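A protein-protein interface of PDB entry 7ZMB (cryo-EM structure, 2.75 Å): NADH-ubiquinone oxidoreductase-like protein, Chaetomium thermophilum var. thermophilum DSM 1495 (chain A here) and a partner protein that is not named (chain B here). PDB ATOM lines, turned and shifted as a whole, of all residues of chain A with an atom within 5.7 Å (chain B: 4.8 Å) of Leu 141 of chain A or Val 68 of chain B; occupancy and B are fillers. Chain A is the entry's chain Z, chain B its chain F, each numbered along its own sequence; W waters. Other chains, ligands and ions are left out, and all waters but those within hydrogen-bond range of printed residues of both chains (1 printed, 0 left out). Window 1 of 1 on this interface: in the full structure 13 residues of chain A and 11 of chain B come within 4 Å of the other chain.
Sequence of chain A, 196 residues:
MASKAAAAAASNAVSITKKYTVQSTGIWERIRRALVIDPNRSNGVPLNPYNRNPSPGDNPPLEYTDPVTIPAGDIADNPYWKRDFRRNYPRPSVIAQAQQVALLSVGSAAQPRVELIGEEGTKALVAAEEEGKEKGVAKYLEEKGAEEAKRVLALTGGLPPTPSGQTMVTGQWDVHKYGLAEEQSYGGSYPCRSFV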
ATOM      1  N   LEU A 104      24.546 -14.977 -11.017  1.00  0.00           N
ATOM      2  CA  LEU A 104      25.293 -16.190 -11.320  1.00  0.00           C
ATOM      3  C   LEU A 104      25.348 -16.471 -12.817  1.00  0.00           C
ATOM      4  O   LEU A 104      26.304 -17.088 -13.290  1.00  0.00           O
ATOM      5  CB  LEU A 104      24.670 -17.377 -10.586  1.00  0.00           C
ATOM      6  CG  LEU A 104      24.847 -17.408  -9.072  1.00  0.00           C
ATOM      7  CD1 LEU A 104      24.596 -18.805  -8.535  1.00  0.00           C
ATOM      8  CD2 LEU A 104      26.229 -16.910  -8.683  1.00  0.00           C
ATOM      9  N   GLY A 136      14.288 -20.696  -9.756  1.00  0.00           N
ATOM     10  CA  GLY A 136      15.065 -20.079  -8.703  1.00  0.00           C
ATOM     11  C   GLY A 136      16.453 -20.664  -8.548  1.00  0.00           C
ATOM     12  O   GLY A 136      16.999 -21.304  -9.449  1.00  0.00           O
ATOM     13  N   VAL A 137      17.026 -20.431  -7.368  1.00  0.00           N
ATOM     14  CA  VAL A 137      18.421 -20.777  -7.121  1.00  0.00           C
ATOM     15  C   VAL A 137      18.605 -22.288  -7.034  1.00  0.00           C
ATOM     16  O   VAL A 137      19.538 -22.847  -7.621  1.00  0.00           O
ATOM     17  CB  VAL A 137      18.910 -20.056  -5.856  1.00  0.00           C
ATOM     18  CG1 VAL A 137      20.248 -20.598  -5.390  1.00  0.00           C
ATOM     19  CG2 VAL A 137      18.994 -18.558  -6.121  1.00  0.00           C
ATOM     20  N   ALA A 138      17.719 -22.974  -6.314  1.00  0.00           N
ATOM     21  CA  ALA A 138      17.836 -24.421  -6.183  1.00  0.00           C
ATOM     22  C   ALA A 138      17.725 -25.116  -7.533  1.00  0.00           C
ATOM     23  O   ALA A 138      18.486 -26.045  -7.824  1.00  0.00           O
ATOM     24  CB  ALA A 138      16.772 -24.950  -5.227  1.00  0.00           C
ATOM     25  N   LYS A 139      16.778 -24.688  -8.365  1.00  0.00           N
ATOM     26  CA  LYS A 139      16.667 -25.238  -9.710  1.00  0.00           C
ATOM     27  C   LYS A 139      17.885 -24.887 -10.554  1.00  0.00           C
ATOM     28  O   LYS A 139      18.347 -25.706 -11.352  1.00  0.00           O
ATOM     29  CB  LYS A 139      15.390 -24.722 -10.369  1.00  0.00           C
ATOM     30  CG  LYS A 139      15.113 -25.276 -11.749  1.00  0.00           C
ATOM     31  CD  LYS A 139      14.803 -26.760 -11.695  1.00  0.00           C
ATOM     32  CE  LYS A 139      13.500 -27.016 -10.949  1.00  0.00           C
ATOM     33  NZ  LYS A 139      12.316 -26.477 -11.675  1.00  0.00           N
ATOM     34  N   TYR A 140      18.408 -23.668 -10.406  1.00  0.00           N
ATOM     35  CA  TYR A 140      19.584 -23.252 -11.168  1.00  0.00           C
ATOM     36  C   TYR A 140      20.787 -24.133 -10.873  1.00  0.00           C
ATOM     37  O   TYR A 140      21.514 -24.535 -11.786  1.00  0.00           O
ATOM     38  CB  TYR A 140      19.931 -21.795 -10.861  1.00  0.00           C
ATOM     39  CG  TYR A 140      20.865 -21.195 -11.866  1.00  0.00           C
ATOM     40  CD1 TYR A 140      20.426 -20.872 -13.135  1.00  0.00           C
ATOM     41  CD2 TYR A 140      22.208 -20.988 -11.558  1.00  0.00           C
ATOM     42  CE1 TYR A 140      21.276 -20.333 -14.057  1.00  0.00           C
ATOM     43  CE2 TYR A 140      23.074 -20.450 -12.480  1.00  0.00           C
ATOM     44  CZ  TYR A 140      22.600 -20.122 -13.731  1.00  0.00           C
ATOM     45  OH  TYR A 140      23.445 -19.582 -14.670  1.00  0.00           O
ATOM     46  N   LEU A 141      21.034 -24.411  -9.597  1.00  0.00           N
ATOM     47  CA  LEU A 141      22.130 -25.295  -9.230  1.00  0.00           C
ATOM     48  C   LEU A 141      21.855 -26.735  -9.610  1.00  0.00           C
ATOM     49  O   LEU A 141      22.798 -27.510  -9.782  1.00  0.00           O
ATOM     50  CB  LEU A 141      22.401 -25.199  -7.734  1.00  0.00           C
ATOM     51  CG  LEU A 141      22.680 -23.786  -7.253  1.00  0.00           C
ATOM     52  CD1 LEU A 141      22.882 -23.806  -5.765  1.00  0.00           C
ATOM     53  CD2 LEU A 141      23.906 -23.234  -7.961  1.00  0.00           C
ATOM     54  N   GLU A 142      20.589 -27.108  -9.754  1.00  0.00           N
ATOM     55  CA  GLU A 142      20.264 -28.476 -10.131  1.00  0.00           C
ATOM     56  C   GLU A 142      20.766 -28.804 -11.530  1.00  0.00           C
ATOM     57  O   GLU A 142      21.402 -29.841 -11.741  1.00  0.00           O
ATOM     58  CB  GLU A 142      18.758 -28.688 -10.026  1.00  0.00           C
ATOM     59  CG  GLU A 142      18.322 -30.103 -10.290  1.00  0.00           C
ATOM     60  CD  GLU A 142      18.790 -31.064  -9.228  1.00  0.00           C
ATOM     61  OE1 GLU A 142      18.999 -30.626  -8.081  1.00  0.00           O
ATOM     62  OE2 GLU A 142      18.950 -32.262  -9.542  1.00  0.00           O
ATOM     63  N   GLU A 143      20.495 -27.931 -12.500  1.00  0.00           N
ATOM     64  CA  GLU A 143      20.811 -28.253 -13.887  1.00  0.00           C
ATOM     65  C   GLU A 143      22.261 -27.941 -14.251  1.00  0.00           C
ATOM     66  O   GLU A 143      22.892 -28.719 -14.973  1.00  0.00           O
ATOM     67  CB  GLU A 143      19.789 -27.580 -14.806  1.00  0.00           C
ATOM     68  CG  GLU A 143      19.795 -26.075 -14.863  1.00  0.00           C
ATOM     69  CD  GLU A 143      20.861 -25.494 -15.741  1.00  0.00           C
ATOM     70  OE1 GLU A 143      21.345 -26.200 -16.646  1.00  0.00           O
ATOM     71  OE2 GLU A 143      21.181 -24.306 -15.540  1.00  0.00           O
ATOM     72  N   LYS A 144      22.824 -26.834 -13.765  1.00  0.00           N
ATOM     73  CA  LYS A 144      24.263 -26.642 -13.922  1.00  0.00           C
ATOM     74  C   LYS A 144      25.105 -27.658 -13.161  1.00  0.00           C
ATOM     75  O   LYS A 144      26.313 -27.732 -13.411  1.00  0.00           O
ATOM     76  CB  LYS A 144      24.667 -25.232 -13.507  1.00  0.00           C
ATOM     77  CG  LYS A 144      24.085 -24.059 -14.283  1.00  0.00           C
ATOM     78  CD  LYS A 144      24.698 -23.955 -15.688  1.00  0.00           C
ATOM     79  CE  LYS A 144      23.932 -24.650 -16.789  1.00  0.00           C
ATOM     80  NZ  LYS A 144      24.531 -24.414 -18.136  1.00  0.00           N
ATOM     81  N   GLY A 145      24.526 -28.422 -12.245  1.00  0.00           N
ATOM     82  CA  GLY A 145      25.291 -29.424 -11.533  1.00  0.00           C
ATOM     83  C   GLY A 145      26.004 -28.852 -10.326  1.00  0.00           C
ATOM     84  O   GLY A 145      25.661 -27.791  -9.801  1.00  0.00           O
ATOM     85  N   ALA A 146      27.037 -29.569  -9.897  1.00  0.00           N
ATOM     86  CA  ALA A 146      27.740 -29.244  -8.666  1.00  0.00           C
ATOM     87  C   ALA A 146      28.855 -28.228  -8.841  1.00  0.00           C
ATOM     88  O   ALA A 146      29.278 -27.623  -7.849  1.00  0.00           O
ATOM     89  CB  ALA A 146      28.327 -30.516  -8.051  1.00  0.00           C
ATOM     90  N   GLU A 148      28.717 -25.400 -10.606  1.00  0.00           N
ATOM     91  CA  GLU A 148      28.151 -24.079 -10.378  1.00  0.00           C
ATOM     92  C   GLU A 148      28.108 -23.771  -8.892  1.00  0.00           C
ATOM     93  O   GLU A 148      28.443 -22.660  -8.466  1.00  0.00           O
ATOM     94  CB  GLU A 148      26.751 -23.998 -10.977  1.00  0.00           C
ATOM     95  CG  GLU A 148      26.073 -22.643 -10.839  1.00  0.00           C
ATOM     96  CD  GLU A 148      26.780 -21.552 -11.615  1.00  0.00           C
ATOM     97  OE1 GLU A 148      27.460 -21.874 -12.611  1.00  0.00           O
ATOM     98  OE2 GLU A 148      26.644 -20.370 -11.235  1.00  0.00           O
ATOM     99  N   ALA A 149      27.697 -24.752  -8.087  1.00  0.00           N
ATOM    100  CA  ALA A 149      27.738 -24.579  -6.645  1.00  0.00           C
ATOM    101  C   ALA A 149      29.164 -24.377  -6.168  1.00  0.00           C
ATOM    102  O   ALA A 149      29.396 -23.684  -5.173  1.00  0.00           O
ATOM    103  CB  ALA A 149      27.101 -25.787  -5.957  1.00  0.00           C
ATOM    104  N   VAL A 152      30.075 -20.872  -6.679  1.00  0.00           N
ATOM    105  CA  VAL A 152      29.492 -20.021  -5.651  1.00  0.00           C
ATOM    106  C   VAL A 152      30.506 -19.780  -4.549  1.00  0.00           C
ATOM    107  O   VAL A 152      30.681 -18.651  -4.076  1.00  0.00           O
ATOM    108  CB  VAL A 152      28.194 -20.652  -5.110  1.00  0.00           C
ATOM    109  CG1 VAL A 152      27.650 -19.862  -3.924  1.00  0.00           C
ATOM    110  CG2 VAL A 152      27.155 -20.758  -6.205  1.00  0.00           C
ATOM    111  N   LEU A 153      31.196 -20.836  -4.125  1.00  0.00           N
ATOM    112  CA  LEU A 153      32.266 -20.676  -3.152  1.00  0.00           C
ATOM    113  C   LEU A 153      33.454 -19.938  -3.753  1.00  0.00           C
ATOM    114  O   LEU A 153      34.215 -19.295  -3.024  1.00  0.00           O
ATOM    115  CB  LEU A 153      32.681 -22.040  -2.607  1.00  0.00           C
ATOM    116  CG  LEU A 153      31.776 -22.689  -1.554  1.00  0.00           C
ATOM    117  CD1 LEU A 153      30.480 -23.168  -2.142  1.00  0.00           C
ATOM    118  CD2 LEU A 153      32.485 -23.858  -0.921  1.00  0.00           C
ATOM    119  N   HIS B  66      25.363 -30.798  -5.796  1.00  0.00           N
ATOM    120  CA  HIS B  66      25.096 -29.430  -6.215  1.00  0.00           C
ATOM    121  C   HIS B  66      24.611 -28.548  -5.071  1.00  0.00           C
ATOM    122  O   HIS B  66      24.365 -27.360  -5.289  1.00  0.00           O
ATOM    123  CB  HIS B  66      24.076 -29.428  -7.351  1.00  0.00           C
ATOM    124  CG  HIS B  66      22.688 -29.727  -6.899  1.00  0.00           C
ATOM    125  ND1 HIS B  66      22.339 -30.927  -6.325  1.00  0.00           N
ATOM    126  CD2 HIS B  66      21.568 -28.970  -6.897  1.00  0.00           C
ATOM    127  CE1 HIS B  66      21.061 -30.902  -5.999  1.00  0.00           C
ATOM    128  NE2 HIS B  66      20.569 -29.726  -6.337  1.00  0.00           N
ATOM    129  N   SER B  67      24.459 -29.095  -3.868  1.00  0.00           N
ATOM    130  CA  SER B  67      24.130 -28.273  -2.718  1.00  0.00           C
ATOM    131  C   SER B  67      25.340 -27.453  -2.287  1.00  0.00           C
ATOM    132  O   SER B  67      26.417 -27.999  -2.034  1.00  0.00           O
ATOM    133  CB  SER B  67      23.655 -29.141  -1.559  1.00  0.00           C
ATOM    134  OG  SER B  67      23.718 -28.434  -0.334  1.00  0.00           O
ATOM    135  N   VAL B  68      25.156 -26.137  -2.204  1.00  0.00           N
ATOM    136  CA  VAL B  68      26.213 -25.270  -1.701  1.00  0.00           C
ATOM    137  C   VAL B  68      26.442 -25.510  -0.215  1.00  0.00           C
ATOM    138  O   VAL B  68      27.558 -25.336   0.282  1.00  0.00           O
ATOM    139  CB  VAL B  68      25.877 -23.802  -2.009  1.00  0.00           C
ATOM    140  CG1 VAL B  68      26.957 -22.878  -1.484  1.00  0.00           C
ATOM    141  CG2 VAL B  68      25.709 -23.615  -3.492  1.00  0.00           C
ATOM    142  N   TYR B  69      25.407 -25.922   0.514  1.00  0.00           N
ATOM    143  CA  TYR B  69      25.593 -26.305   1.910  1.00  0.00           C
ATOM    144  C   TYR B  69      26.557 -27.474   2.034  1.00  0.00           C
ATOM    145  O   TYR B  69      27.439 -27.481   2.900  1.00  0.00           O
ATOM    146  CB  TYR B  69      24.258 -26.672   2.542  1.00  0.00           C
ATOM    147  CG  TYR B  69      24.418 -27.306   3.899  1.00  0.00           C
ATOM    148  CD1 TYR B  69      24.854 -26.562   4.978  1.00  0.00           C
ATOM    149  CD2 TYR B  69      24.151 -28.648   4.098  1.00  0.00           C
ATOM    150  CE1 TYR B  69      25.000 -27.126   6.214  1.00  0.00           C
ATOM    151  CE2 TYR B  69      24.306 -29.221   5.329  1.00  0.00           C
ATOM    152  CZ  TYR B  69      24.731 -28.455   6.387  1.00  0.00           C
ATOM    153  OH  TYR B  69      24.883 -29.017   7.630  1.00  0.00           O
ATOM    154  N   ARG B  70      26.398 -28.486   1.185  1.00  0.00           N
ATOM    155  CA  ARG B  70      27.342 -29.590   1.208  1.00  0.00           C
ATOM    156  C   ARG B  70      28.743 -29.084   0.901  1.00  0.00           C
ATOM    157  O   ARG B  70      29.670 -29.286   1.692  1.00  0.00           O
ATOM    158  CB  ARG B  70      26.930 -30.663   0.210  1.00  0.00           C
ATOM    159  CG  ARG B  70      27.655 -31.980   0.381  1.00  0.00           C
ATOM    160  CD  ARG B  70      27.195 -32.979  -0.664  1.00  0.00           C
ATOM    161  NE  ARG B  70      27.674 -34.329  -0.401  1.00  0.00           N
ATOM    162  CZ  ARG B  70      28.874 -34.778  -0.730  1.00  0.00           C
ATOM    163  NH1 ARG B  70      29.745 -33.979  -1.325  1.00  0.00           N
ATOM    164  NH2 ARG B  70      29.208 -36.022  -0.447  1.00  0.00           N
ATOM    165  N   GLN B  71      28.897 -28.358  -0.206  1.00  0.00           N
ATOM    166  CA  GLN B  71      30.216 -27.886  -0.595  1.00  0.00           C
ATOM    167  C   GLN B  71      30.839 -26.975   0.446  1.00  0.00           C
ATOM    168  O   GLN B  71      32.060 -26.991   0.597  1.00  0.00           O
ATOM    169  CB  GLN B  71      30.156 -27.165  -1.938  1.00  0.00           C
ATOM    170  CG  GLN B  71      29.594 -27.995  -3.060  1.00  0.00           C
ATOM    171  CD  GLN B  71      30.311 -29.308  -3.226  1.00  0.00           C
ATOM    172  OE1 GLN B  71      31.532 -29.379  -3.101  1.00  0.00           O
ATOM    173  NE2 GLN B  71      29.559 -30.367  -3.500  1.00  0.00           N
ATOM    174  N   SER B  72      30.037 -26.183   1.158  1.00  0.00           N
ATOM    175  CA  SER B  72      30.563 -25.312   2.201  1.00  0.00           C
ATOM    176  C   SER B  72      31.106 -26.120   3.375  1.00  0.00           C
ATOM    177  O   SER B  72      32.279 -26.000   3.738  1.00  0.00           O
ATOM    178  CB  SER B  72      29.471 -24.351   2.672  1.00  0.00           C
ATOM    179  OG  SER B  72      29.178 -23.384   1.689  1.00  0.00           O
HETATM  180  O   HOH W   1      19.981 -26.624  -5.265  1.00  0.00           O
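CB of His 66 of chain B touches O of Leu 141 of chain A, 3.3 Å away.
CG2 of Val 68 of chain B touches CD1 of Leu 141 of chain A, 3.6 Å away.
Gly 145 of chain A touches His 66 of chain B (O to CB, 3.3 Å).
Ala 146 of chain A touches His 66 of chain B.
CB of Ala 149 of chain A touches O of His 66 of chain B, at 3.2 Å.
Ala 149 of chain A touches Val 68 of chain B (CB to CG2, 3.6 Å).
CG1 of Val 152 of chain A touches CG1 of Val 68 of chain B (3.9 Å).
CG1 of Val 68 of chain B touches CD1 of Leu 153 of chain A, 3.6 Å away.
Leu 153 of chain A touches Gln 71 of chain B (CD2 to O, 3.5 Å).
Ser 72 of chain B touches Leu 153 of chain A.
A ring nitrogen (NE2) of His 66 of chain B sits at hydrogen-bond distance from the side-chain carboxylate (OE1) of Glu 142 of chain A.
Printed residues of chain B within 4 Å of Leu 141 of chain A: His 66 (3.3 Å) and Val 68 (3.6 Å).
Printed residues of chain B within 4 Å of Gly 145 of chain A: His 66.
Of the printed residues of chain B, Leu 153 of chain A touches Val 68 (3.6 Å), Gln 71 (3.5 Å) and Ser 72 (3.9 Å).
Printed residues of chain A within 4 Å of His 66 of chain B: Leu 141, Glu 142, Gly 145, Ala 146 and Ala 149.
Of chain A, only Leu 141, Ala 149, Val 152 and Leu 153 come within 4 Å of Val 68 of chain B.
Of the printed residues of chain A, Ser 72 of chain B touches Leu 153.
The nearest printed residue of chain B that does not touch Leu 141 of chain A is Ser 67 of chain B (5.5 Å).
The nearest printed residue of chain A that does not touch Gln 71 of chain B is Ala 149 of chain A (4.4 Å).
O of Val 68 of chain B lies within hydrogen-bond range of OG of Ser 72 of chain B, 2.9 Å away.
Hydrophobic or aromatic side chains of chain A that line the printed part of chain B: Leu 141, Ala 146, Ala 149, Val 152 and Leu 153.
Of the 7 printed residues of chain B, 4 touch a printed residue of chain A.
Hydrophobic or aromatic side chains of chain B that line the printed part of chain A: His 66 and Val 68.
Among the printed residues, 11 pairs touch across the chains.
Among the printed residues, no Asp or Glu carboxylate lies within 4 Å of a Lys or Arg side-chain nitrogen of the other chain.
Water W1 lies within hydrogen-bond range of O of Ala 138 of chain A and NE2 of His 66 of chain B.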
